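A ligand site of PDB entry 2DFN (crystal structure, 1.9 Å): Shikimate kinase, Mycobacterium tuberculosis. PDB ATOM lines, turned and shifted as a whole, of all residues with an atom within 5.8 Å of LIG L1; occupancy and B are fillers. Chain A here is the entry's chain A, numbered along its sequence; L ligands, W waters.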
ATOM      1  N   GLY A   9       1.585 -16.182  17.687  1.00  0.00           N
ATOM      2  CA  GLY A   9       1.993 -16.534  16.346  1.00  0.00           C
ATOM      3  C   GLY A   9       2.183 -15.213  15.628  1.00  0.00           C
ATOM      4  O   GLY A   9       2.115 -14.129  16.244  1.00  0.00           O
ATOM      5  N   LEU A  10       2.544 -15.292  14.357  1.00  0.00           N
ATOM      6  CA  LEU A  10       2.949 -14.080  13.675  1.00  0.00           C
ATOM      7  C   LEU A  10       1.748 -13.175  13.410  1.00  0.00           C
ATOM      8  O   LEU A  10       0.617 -13.594  13.474  1.00  0.00           O
ATOM      9  CB  LEU A  10       3.629 -14.426  12.344  1.00  0.00           C
ATOM     10  CG  LEU A  10       4.930 -15.220  12.486  1.00  0.00           C
ATOM     11  CD1 LEU A  10       5.170 -15.827  11.132  1.00  0.00           C
ATOM     12  CD2 LEU A  10       6.009 -14.107  12.815  1.00  0.00           C
ATOM     13  N   PRO A  11       1.994 -11.901  13.100  1.00  0.00           N
ATOM     14  CA  PRO A  11       0.915 -11.031  12.643  1.00  0.00           C
ATOM     15  C   PRO A  11       0.167 -11.724  11.521  1.00  0.00           C
ATOM     16  O   PRO A  11       0.780 -12.372  10.672  1.00  0.00           O
ATOM     17  CB  PRO A  11       1.655  -9.846  12.036  1.00  0.00           C
ATOM     18  CG  PRO A  11       3.124 -10.124  12.238  1.00  0.00           C
ATOM     19  CD  PRO A  11       3.310 -11.263  13.132  1.00  0.00           C
ATOM     20  N   GLY A  12      -1.156 -11.626  11.582  1.00  0.00           N
ATOM     21  CA  GLY A  12      -2.025 -12.288  10.626  1.00  0.00           C
ATOM     22  C   GLY A  12      -2.174 -13.792  10.704  1.00  0.00           C
ATOM     23  O   GLY A  12      -2.846 -14.376   9.857  1.00  0.00           O
ATOM     24  N   SER A  13      -1.592 -14.457  11.711  1.00  0.00           N
ATOM     25  CA  SER A  13      -1.809 -15.886  11.917  1.00  0.00           C
ATOM     26  C   SER A  13      -3.249 -16.255  12.390  1.00  0.00           C
ATOM     27  O   SER A  13      -3.625 -17.429  12.362  1.00  0.00           O
ATOM     28  CB  SER A  13      -0.767 -16.468  12.915  1.00  0.00           C
ATOM     29  OG  SER A  13      -0.819 -15.842  14.208  1.00  0.00           O
ATOM     30  N   GLY A  14      -4.001 -15.271  12.848  1.00  0.00           N
ATOM     31  CA  GLY A  14      -5.355 -15.427  13.344  1.00  0.00           C
ATOM     32  C   GLY A  14      -5.533 -15.171  14.844  1.00  0.00           C
ATOM     33  O   GLY A  14      -6.607 -15.495  15.361  1.00  0.00           O
ATOM     34  N   LYS A  15      -4.538 -14.637  15.570  1.00  0.00           N
ATOM     35  CA  LYS A  15      -4.642 -14.486  17.070  1.00  0.00           C
ATOM     36  C   LYS A  15      -5.954 -13.787  17.484  1.00  0.00           C
ATOM     37  O   LYS A  15      -6.704 -14.254  18.372  1.00  0.00           O
ATOM     38  CB  LYS A  15      -3.428 -13.710  17.691  1.00  0.00           C
ATOM     39  CG  LYS A  15      -2.088 -14.506  17.614  1.00  0.00           C
ATOM     40  CD  LYS A  15      -0.846 -13.713  18.147  1.00  0.00           C
ATOM     41  CE  LYS A  15      -0.741 -12.314  17.548  1.00  0.00           C
ATOM     42  NZ  LYS A  15      -0.645 -12.302  16.034  1.00  0.00           N
ATOM     43  N   SER A  16      -6.210 -12.641  16.865  1.00  0.00           N
ATOM     44  CA  SER A  16      -7.381 -11.826  17.208  1.00  0.00           C
ATOM     45  C   SER A  16      -8.681 -12.474  16.746  1.00  0.00           C
ATOM     46  O   SER A  16      -9.664 -12.479  17.479  1.00  0.00           O
ATOM     47  CB  SER A  16      -7.256 -10.404  16.665  1.00  0.00           C
ATOM     48  OG  SER A  16      -6.243  -9.721  17.388  1.00  0.00           O
ATOM     49  N   THR A  17      -8.665 -13.077  15.547  1.00  0.00           N
ATOM     50  CA  THR A  17      -9.830 -13.689  14.935  1.00  0.00           C
ATOM     51  C   THR A  17     -10.164 -15.015  15.576  1.00  0.00           C
ATOM     52  O   THR A  17     -11.301 -15.270  15.979  1.00  0.00           O
ATOM     53  CB  THR A  17      -9.586 -14.004  13.420  1.00  0.00           C
ATOM     54  OG1 THR A  17      -9.330 -12.767  12.765  1.00  0.00           O
ATOM     55  CG2 THR A  17     -10.872 -14.640  12.789  1.00  0.00           C
ATOM     56  N   ILE A  18      -9.154 -15.857  15.684  1.00  0.00           N
ATOM     57  CA  ILE A  18      -9.359 -17.153  16.291  1.00  0.00           C
ATOM     58  C   ILE A  18      -9.653 -16.944  17.778  1.00  0.00           C
ATOM     59  O   ILE A  18     -10.538 -17.618  18.336  1.00  0.00           O
ATOM     60  CB  ILE A  18      -8.116 -18.015  16.158  1.00  0.00           C
ATOM     61  CG1 ILE A  18      -7.801 -18.259  14.685  1.00  0.00           C
ATOM     62  CG2 ILE A  18      -8.349 -19.318  16.855  1.00  0.00           C
ATOM     63  CD1 ILE A  18      -8.866 -19.092  14.005  1.00  0.00           C
ATOM     64  N   ASP A  32      -7.432  -9.286  24.355  1.00  0.00           N
ATOM     65  CA  ASP A  32      -6.484  -9.153  23.289  1.00  0.00           C
ATOM     66  C   ASP A  32      -5.495  -8.133  23.812  1.00  0.00           C
ATOM     67  O   ASP A  32      -5.852  -6.981  24.030  1.00  0.00           O
ATOM     68  CB  ASP A  32      -7.172  -8.686  21.986  1.00  0.00           C
ATOM     69  CG  ASP A  32      -6.171  -8.541  20.847  1.00  0.00           C
ATOM     70  OD1 ASP A  32      -4.970  -8.229  21.083  1.00  0.00           O
ATOM     71  OD2 ASP A  32      -6.564  -8.749  19.705  1.00  0.00           O
ATOM     72  N   LEU A 100      -0.540 -20.564  16.578  1.00  0.00           N
ATOM     73  CA  LEU A 100      -1.084 -20.525  15.228  1.00  0.00           C
ATOM     74  C   LEU A 100       0.034 -20.328  14.188  1.00  0.00           C
ATOM     75  O   LEU A 100       0.691 -19.260  14.113  1.00  0.00           O
ATOM     76  CB  LEU A 100      -2.145 -19.445  15.103  1.00  0.00           C
ATOM     77  CG  LEU A 100      -3.233 -19.402  16.212  1.00  0.00           C
ATOM     78  CD1 LEU A 100      -4.060 -18.121  15.941  1.00  0.00           C
ATOM     79  CD2 LEU A 100      -4.175 -20.605  16.193  1.00  0.00           C
ATOM     80  N   GLU A 106       1.019 -16.862   2.820  1.00  0.00           N
ATOM     81  CA  GLU A 106      -0.331 -16.672   3.318  1.00  0.00           C
ATOM     82  C   GLU A 106      -0.421 -15.551   4.344  1.00  0.00           C
ATOM     83  O   GLU A 106      -1.370 -14.747   4.322  1.00  0.00           O
ATOM     84  CB  GLU A 106      -0.934 -17.974   3.826  1.00  0.00           C
ATOM     85  CG  GLU A 106      -2.381 -17.770   4.379  1.00  0.00           C
ATOM     86  CD  GLU A 106      -3.376 -17.242   3.320  1.00  0.00           C
ATOM     87  OE1 GLU A 106      -3.203 -17.510   2.117  1.00  0.00           O
ATOM     88  OE2 GLU A 106      -4.330 -16.547   3.733  1.00  0.00           O
ATOM     89  N   ARG A 110      -2.621 -12.243   4.311  1.00  0.00           N
ATOM     90  CA  ARG A 110      -3.685 -12.065   5.295  1.00  0.00           C
ATOM     91  C   ARG A 110      -3.546 -10.681   5.888  1.00  0.00           C
ATOM     92  O   ARG A 110      -4.559 -10.019   6.145  1.00  0.00           O
ATOM     93  CB  ARG A 110      -3.653 -13.136   6.408  1.00  0.00           C
ATOM     94  CG  ARG A 110      -4.270 -14.455   6.053  1.00  0.00           C
ATOM     95  CD  ARG A 110      -4.424 -15.316   7.301  1.00  0.00           C
ATOM     96  NE  ARG A 110      -4.652 -16.707   6.931  1.00  0.00           N
ATOM     97  CZ  ARG A 110      -4.581 -17.717   7.784  1.00  0.00           C
ATOM     98  NH1 ARG A 110      -4.281 -17.487   9.058  1.00  0.00           N
ATOM     99  NH2 ARG A 110      -4.758 -18.958   7.370  1.00  0.00           N
ATOM    100  N   THR A 111      -2.296 -10.218   6.043  1.00  0.00           N
ATOM    101  CA  THR A 111      -1.989  -8.886   6.565  1.00  0.00           C
ATOM    102  C   THR A 111      -1.969  -7.755   5.526  1.00  0.00           C
ATOM    103  O   THR A 111      -1.472  -6.671   5.830  1.00  0.00           O
ATOM    104  CB  THR A 111      -0.628  -8.838   7.324  1.00  0.00           C
ATOM    105  OG1 THR A 111       0.480  -9.146   6.448  1.00  0.00           O
ATOM    106  CG2 THR A 111      -0.606  -9.779   8.521  1.00  0.00           C
ATOM    107  N   ARG A 117       0.092  -2.480  11.777  1.00  0.00           N
ATOM    108  CA  ARG A 117       1.379  -3.148  11.987  1.00  0.00           C
ATOM    109  C   ARG A 117       2.701  -2.406  11.729  1.00  0.00           C
ATOM    110  O   ARG A 117       3.304  -2.564  10.664  1.00  0.00           O
ATOM    111  CB  ARG A 117       1.341  -4.593  11.485  1.00  0.00           C
ATOM    112  CG  ARG A 117       0.381  -5.491  12.315  1.00  0.00           C
ATOM    113  CD  ARG A 117       0.299  -6.919  11.792  1.00  0.00           C
ATOM    114  NE  ARG A 117      -0.903  -7.690  12.138  1.00  0.00           N
ATOM    115  CZ  ARG A 117      -1.959  -7.834  11.340  1.00  0.00           C
ATOM    116  NH1 ARG A 117      -2.004  -7.186  10.171  1.00  0.00           N
ATOM    117  NH2 ARG A 117      -3.006  -8.579  11.729  1.00  0.00           N
ATOM    118  N   THR A 150      -2.650 -23.302  10.538  1.00  0.00           N
ATOM    119  CA  THR A 150      -3.818 -22.570  10.092  1.00  0.00           C
ATOM    120  C   THR A 150      -3.811 -22.347   8.579  1.00  0.00           C
ATOM    121  O   THR A 150      -4.641 -21.597   8.030  1.00  0.00           O
ATOM    122  CB  THR A 150      -3.903 -21.233  10.740  1.00  0.00           C
ATOM    123  OG1 THR A 150      -2.940 -20.359  10.147  1.00  0.00           O
ATOM    124  CG2 THR A 150      -3.693 -21.376  12.327  1.00  0.00           C
ATOM    125  N   ARG A 153      -6.607 -24.249   6.797  1.00  0.00           N
ATOM    126  CA  ARG A 153      -7.724 -24.509   7.708  1.00  0.00           C
ATOM    127  C   ARG A 153      -8.477 -23.196   7.796  1.00  0.00           C
ATOM    128  O   ARG A 153      -7.867 -22.141   7.991  1.00  0.00           O
ATOM    129  CB  ARG A 153      -7.256 -24.874   9.128  1.00  0.00           C
ATOM    130  CG  ARG A 153      -7.009 -26.337   9.424  1.00  0.00           C
ATOM    131  CD  ARG A 153      -6.993 -26.628  10.955  1.00  0.00           C
ATOM    132  NE  ARG A 153      -6.683 -28.033  11.199  1.00  0.00           N
ATOM    133  CZ  ARG A 153      -5.471 -28.494  11.489  1.00  0.00           C
ATOM    134  NH1 ARG A 153      -4.436 -27.666  11.592  1.00  0.00           N
ATOM    135  NH2 ARG A 153      -5.306 -29.807  11.650  1.00  0.00           N
ATOM    136  N   ASN A 154      -9.791 -23.250   7.706  1.00  0.00           N
ATOM    137  CA  ASN A 154     -10.566 -22.030   7.824  1.00  0.00           C
ATOM    138  C   ASN A 154     -10.733 -21.731   9.320  1.00  0.00           C
ATOM    139  O   ASN A 154     -10.427 -22.612  10.126  1.00  0.00           O
ATOM    140  CB  ASN A 154     -11.875 -22.174   7.066  1.00  0.00           C
ATOM    141  CG  ASN A 154     -12.752 -23.279   7.590  1.00  0.00           C
ATOM    142  OD1 ASN A 154     -12.937 -23.424   8.802  1.00  0.00           O
ATOM    143  ND2 ASN A 154     -13.326 -24.069   6.665  1.00  0.00           N
ATOM    144  N   PRO A 155     -11.114 -20.484   9.699  1.00  0.00           N
ATOM    145  CA  PRO A 155     -11.091 -20.121  11.124  1.00  0.00           C
ATOM    146  C   PRO A 155     -11.916 -21.050  12.014  1.00  0.00           C
ATOM    147  O   PRO A 155     -11.414 -21.445  13.069  1.00  0.00           O
ATOM    148  CB  PRO A 155     -11.581 -18.669  11.161  1.00  0.00           C
ATOM    149  CG  PRO A 155     -11.251 -18.191   9.694  1.00  0.00           C
ATOM    150  CD  PRO A 155     -11.563 -19.368   8.854  1.00  0.00           C
ATOM    151  N   VAL A 158      -9.960 -24.205  12.626  1.00  0.00           N
ATOM    152  CA  VAL A 158      -8.865 -23.945  13.581  1.00  0.00           C
ATOM    153  C   VAL A 158      -9.430 -23.935  15.010  1.00  0.00           C
ATOM    154  O   VAL A 158      -8.894 -24.661  15.849  1.00  0.00           O
ATOM    155  CB  VAL A 158      -8.074 -22.621  13.328  1.00  0.00           C
ATOM    156  CG1 VAL A 158      -6.983 -22.405  14.424  1.00  0.00           C
ATOM    157  CG2 VAL A 158      -7.493 -22.623  11.874  1.00  0.00           C
HETATM  158  P1  LIG L   1      -3.384 -11.568  14.219  1.00  0.00           P
HETATM  159  O1  LIG L   1      -2.596 -12.798  14.494  1.00  0.00           O
HETATM  160  O2  LIG L   1      -4.233 -11.273  15.420  1.00  0.00           O
HETATM  161  O3  LIG L   1      -2.636 -10.404  13.611  1.00  0.00           O
HETATM  162  P2  LIG L   1      -5.919 -11.592  12.764  1.00  0.00           P
HETATM  163  O4  LIG L   1      -6.008 -10.095  12.781  1.00  0.00           O
HETATM  164  O5  LIG L   1      -6.846 -12.409  13.604  1.00  0.00           O
HETATM  165  O6  LIG L   1      -4.387 -12.046  13.022  1.00  0.00           O
HETATM  166  O7  LIG L   1      -6.168 -12.174  11.278  1.00  0.00           O
HETATM  167  C1  LIG L   1      -5.679 -11.472  10.123  1.00  0.00           C
HETATM  168  C2  LIG L   1      -6.671 -11.610   8.978  1.00  0.00           C
HETATM  169  O8  LIG L   1      -6.550 -12.939   8.500  1.00  0.00           O
HETATM  170  C3  LIG L   1      -8.131 -11.374   9.399  1.00  0.00           C
HETATM  171  O9  LIG L   1      -8.901 -10.770   8.356  1.00  0.00           O
HETATM  172  C4  LIG L   1      -8.723 -12.753   9.526  1.00  0.00           C
HETATM  173  O10 LIG L   1     -10.033 -12.611   8.991  1.00  0.00           O
HETATM  174  C5  LIG L   1      -7.812 -13.594   8.616  1.00  0.00           C
HETATM  175  N1  LIG L   1      -7.664 -14.956   9.126  1.00  0.00           N
HETATM  176  C6  LIG L   1      -7.320 -15.299  10.380  1.00  0.00           C
HETATM  177  N2  LIG L   1      -7.251 -16.632  10.476  1.00  0.00           N
HETATM  178  C7  LIG L   1      -7.649 -17.139   9.285  1.00  0.00           C
HETATM  179  C8  LIG L   1      -7.858 -18.506   8.740  1.00  0.00           C
HETATM  180  N3  LIG L   1      -7.701 -19.654   9.432  1.00  0.00           N
HETATM  181  N4  LIG L   1      -8.243 -18.579   7.440  1.00  0.00           N
HETATM  182  C9  LIG L   1      -8.503 -17.478   6.730  1.00  0.00           C
HETATM  183  N5  LIG L   1      -8.286 -16.197   7.084  1.00  0.00           N
HETATM  184  C10 LIG L   1      -7.897 -16.015   8.372  1.00  0.00           C
HETATM  185  O1  LG2 L   2       1.412  -5.985  19.033  1.00  0.00           O
HETATM  186  C1  LG2 L   2       1.200  -5.648  17.663  1.00  0.00           C
HETATM  187  C2  LG2 L   2       1.072  -6.907  16.777  1.00  0.00           C
HETATM  188  O2  LG2 L   2       0.142  -7.967  17.162  1.00  0.00           O
HETATM  189  C3  LG2 L   2       2.385  -7.238  16.066  1.00  0.00           C
HETATM  190  C4  LG2 L   2       3.586  -6.879  16.548  1.00  0.00           C
HETATM  191  C5  LG2 L   2       4.702  -7.580  16.280  1.00  0.00           C
HETATM  192  O3  LG2 L   2       5.756  -7.214  16.843  1.00  0.00           O
HETATM  193  O4  LG2 L   2       4.720  -8.549  15.500  1.00  0.00           O
HETATM  194  C6  LG2 L   2       3.628  -5.796  17.363  1.00  0.00           C
HETATM  195  C7  LG2 L   2       2.449  -4.836  17.286  1.00  0.00           C
HETATM  196  O5  LG2 L   2       2.289  -4.213  16.002  1.00  0.00           O
HETATM  197  O   HOH W   1      -5.079  -8.419  14.602  1.00  0.00           O
HETATM  198  O   HOH W   2      -2.187  -7.253  14.743  1.00  0.00           O
HETATM  199  O   HOH W   3      -9.128 -20.343   5.302  1.00  0.00           O
HETATM  200  O   HOH W   4      -3.324  -9.027  17.299  1.00  0.00           O
HETATM  201  O   HOH W   5     -11.291 -15.216   9.029  1.00  0.00           O
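The backbone NH (N) of Lys 15 is in hydrogen-bond range of an oxygen (O1) of LIG L1. An oxygen (O1) of LIG L1 is in salt-bridge range of the side-chain amino group (NZ) of Lys 15, at 2.5 Å. N of Thr 17 sits at hydrogen-bond distance from O5 of LIG L1 (2.7 Å). An oxygen (O5) of LIG L1 lies within hydrogen-bond range of the side-chain hydroxyl (OG1) of Thr 17 (2.6 Å). NH2 of Arg 117 is in salt-bridge range of O3 of LIG L1 (2.6 Å). An oxygen (O3) of LIG L1 is in hydrogen-bond range of the backbone NH (N) of Gly 12 (2.8 Å). The backbone NH of Ser 16 sits at hydrogen-bond distance from an oxygen (O2) of LIG L1 (2.8 Å). The side-chain hydroxyl (OG) of Ser 16 lies within hydrogen-bond range of an oxygen (O2) of LIG L1, at 3.2 Å. The backbone carbonyl oxygen of Arg 153 sits at hydrogen-bond distance from a nitrogen (N3) of LIG L1, 2.9 Å away. The backbone NH (N) of Gly 14 sits at hydrogen-bond distance from an oxygen (O6) of LIG L1 (3.3 Å). The backbone NH (N) of Ser 13 sits at hydrogen-bond distance from an oxygen (O1) of LIG L1, at 3.4 Å. N2 of LIG L1 lies close to NH1 of Arg 110 (3.4 Å).
An oxygen (O1) of LIG L1 sits close to the backbone carbonyl oxygen (O) of Leu 10, 3.5 Å away. Pro 11 touches LIG L1 (CA to O3, 3.7 Å). Thr 150 touches LIG L1. Asn 154 touches LIG L1 (C to N3, 3.7 Å). Pro 155 touches LIG L1. Val 158 touches LIG L1. Hydrophobic or aromatic side chains that line LIG L1: Pro 155 and Val 158. 15 residues have an atom within 4 Å of LIG L1: Leu 10, Pro 11, Gly 12, Ser 13, Gly 14, Lys 15, Ser 16, Thr 17, Arg 110, Arg 117, Thr 150, Arg 153, Asn 154, Pro 155 and Val 158.
Water W1 lies within hydrogen-bond range of an oxygen (O4) of LIG L1 (2.6 Å) and the side-chain hydroxyl (OG) of Ser 16 (3.3 Å). Water W3 lies within hydrogen-bond range of a nitrogen (N4) of LIG L1 (2.9 Å) and the backbone carbonyl oxygen (O) of Arg 153 (3.5 Å). Water W4 lies within hydrogen-bond range of the side-chain hydroxyl (OG) of Ser 16 (3.0 Å) and an oxygen (O2) of LIG L1 (3.1 Å). Water W2 lies within hydrogen-bond range of the guanidinium group (NE) of Arg 117, an oxygen (O3) of LIG L1 and an oxygen (O2) of LG2 L2.
NZ of Lys 15 is in hydrogen-bond range of O of Leu 10, at 3.1 Å. O of Gly 9 is in hydrogen-bond range of NZ of Lys 15, 3.3 Å away. The side-chain carboxylate (OD2) of Asp 32 is in hydrogen-bond range of the side-chain hydroxyl (OG) of Ser 16, 2.5 Å away. The guanidinium group (NH1) of Arg 110 lies within hydrogen-bond range of the backbone carbonyl oxygen (O) of Ser 13 (3.4 Å). OG of Ser 13 sits at hydrogen-bond distance from O of Leu 10 (2.8 Å). The backbone carbonyl oxygen (O) of Thr 150 lies within hydrogen-bond range of the guanidinium group (NH2) of Arg 110 (2.7 Å). NE of Arg 110 is in salt-bridge range of OE2 of Glu 106 (3.2 Å).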
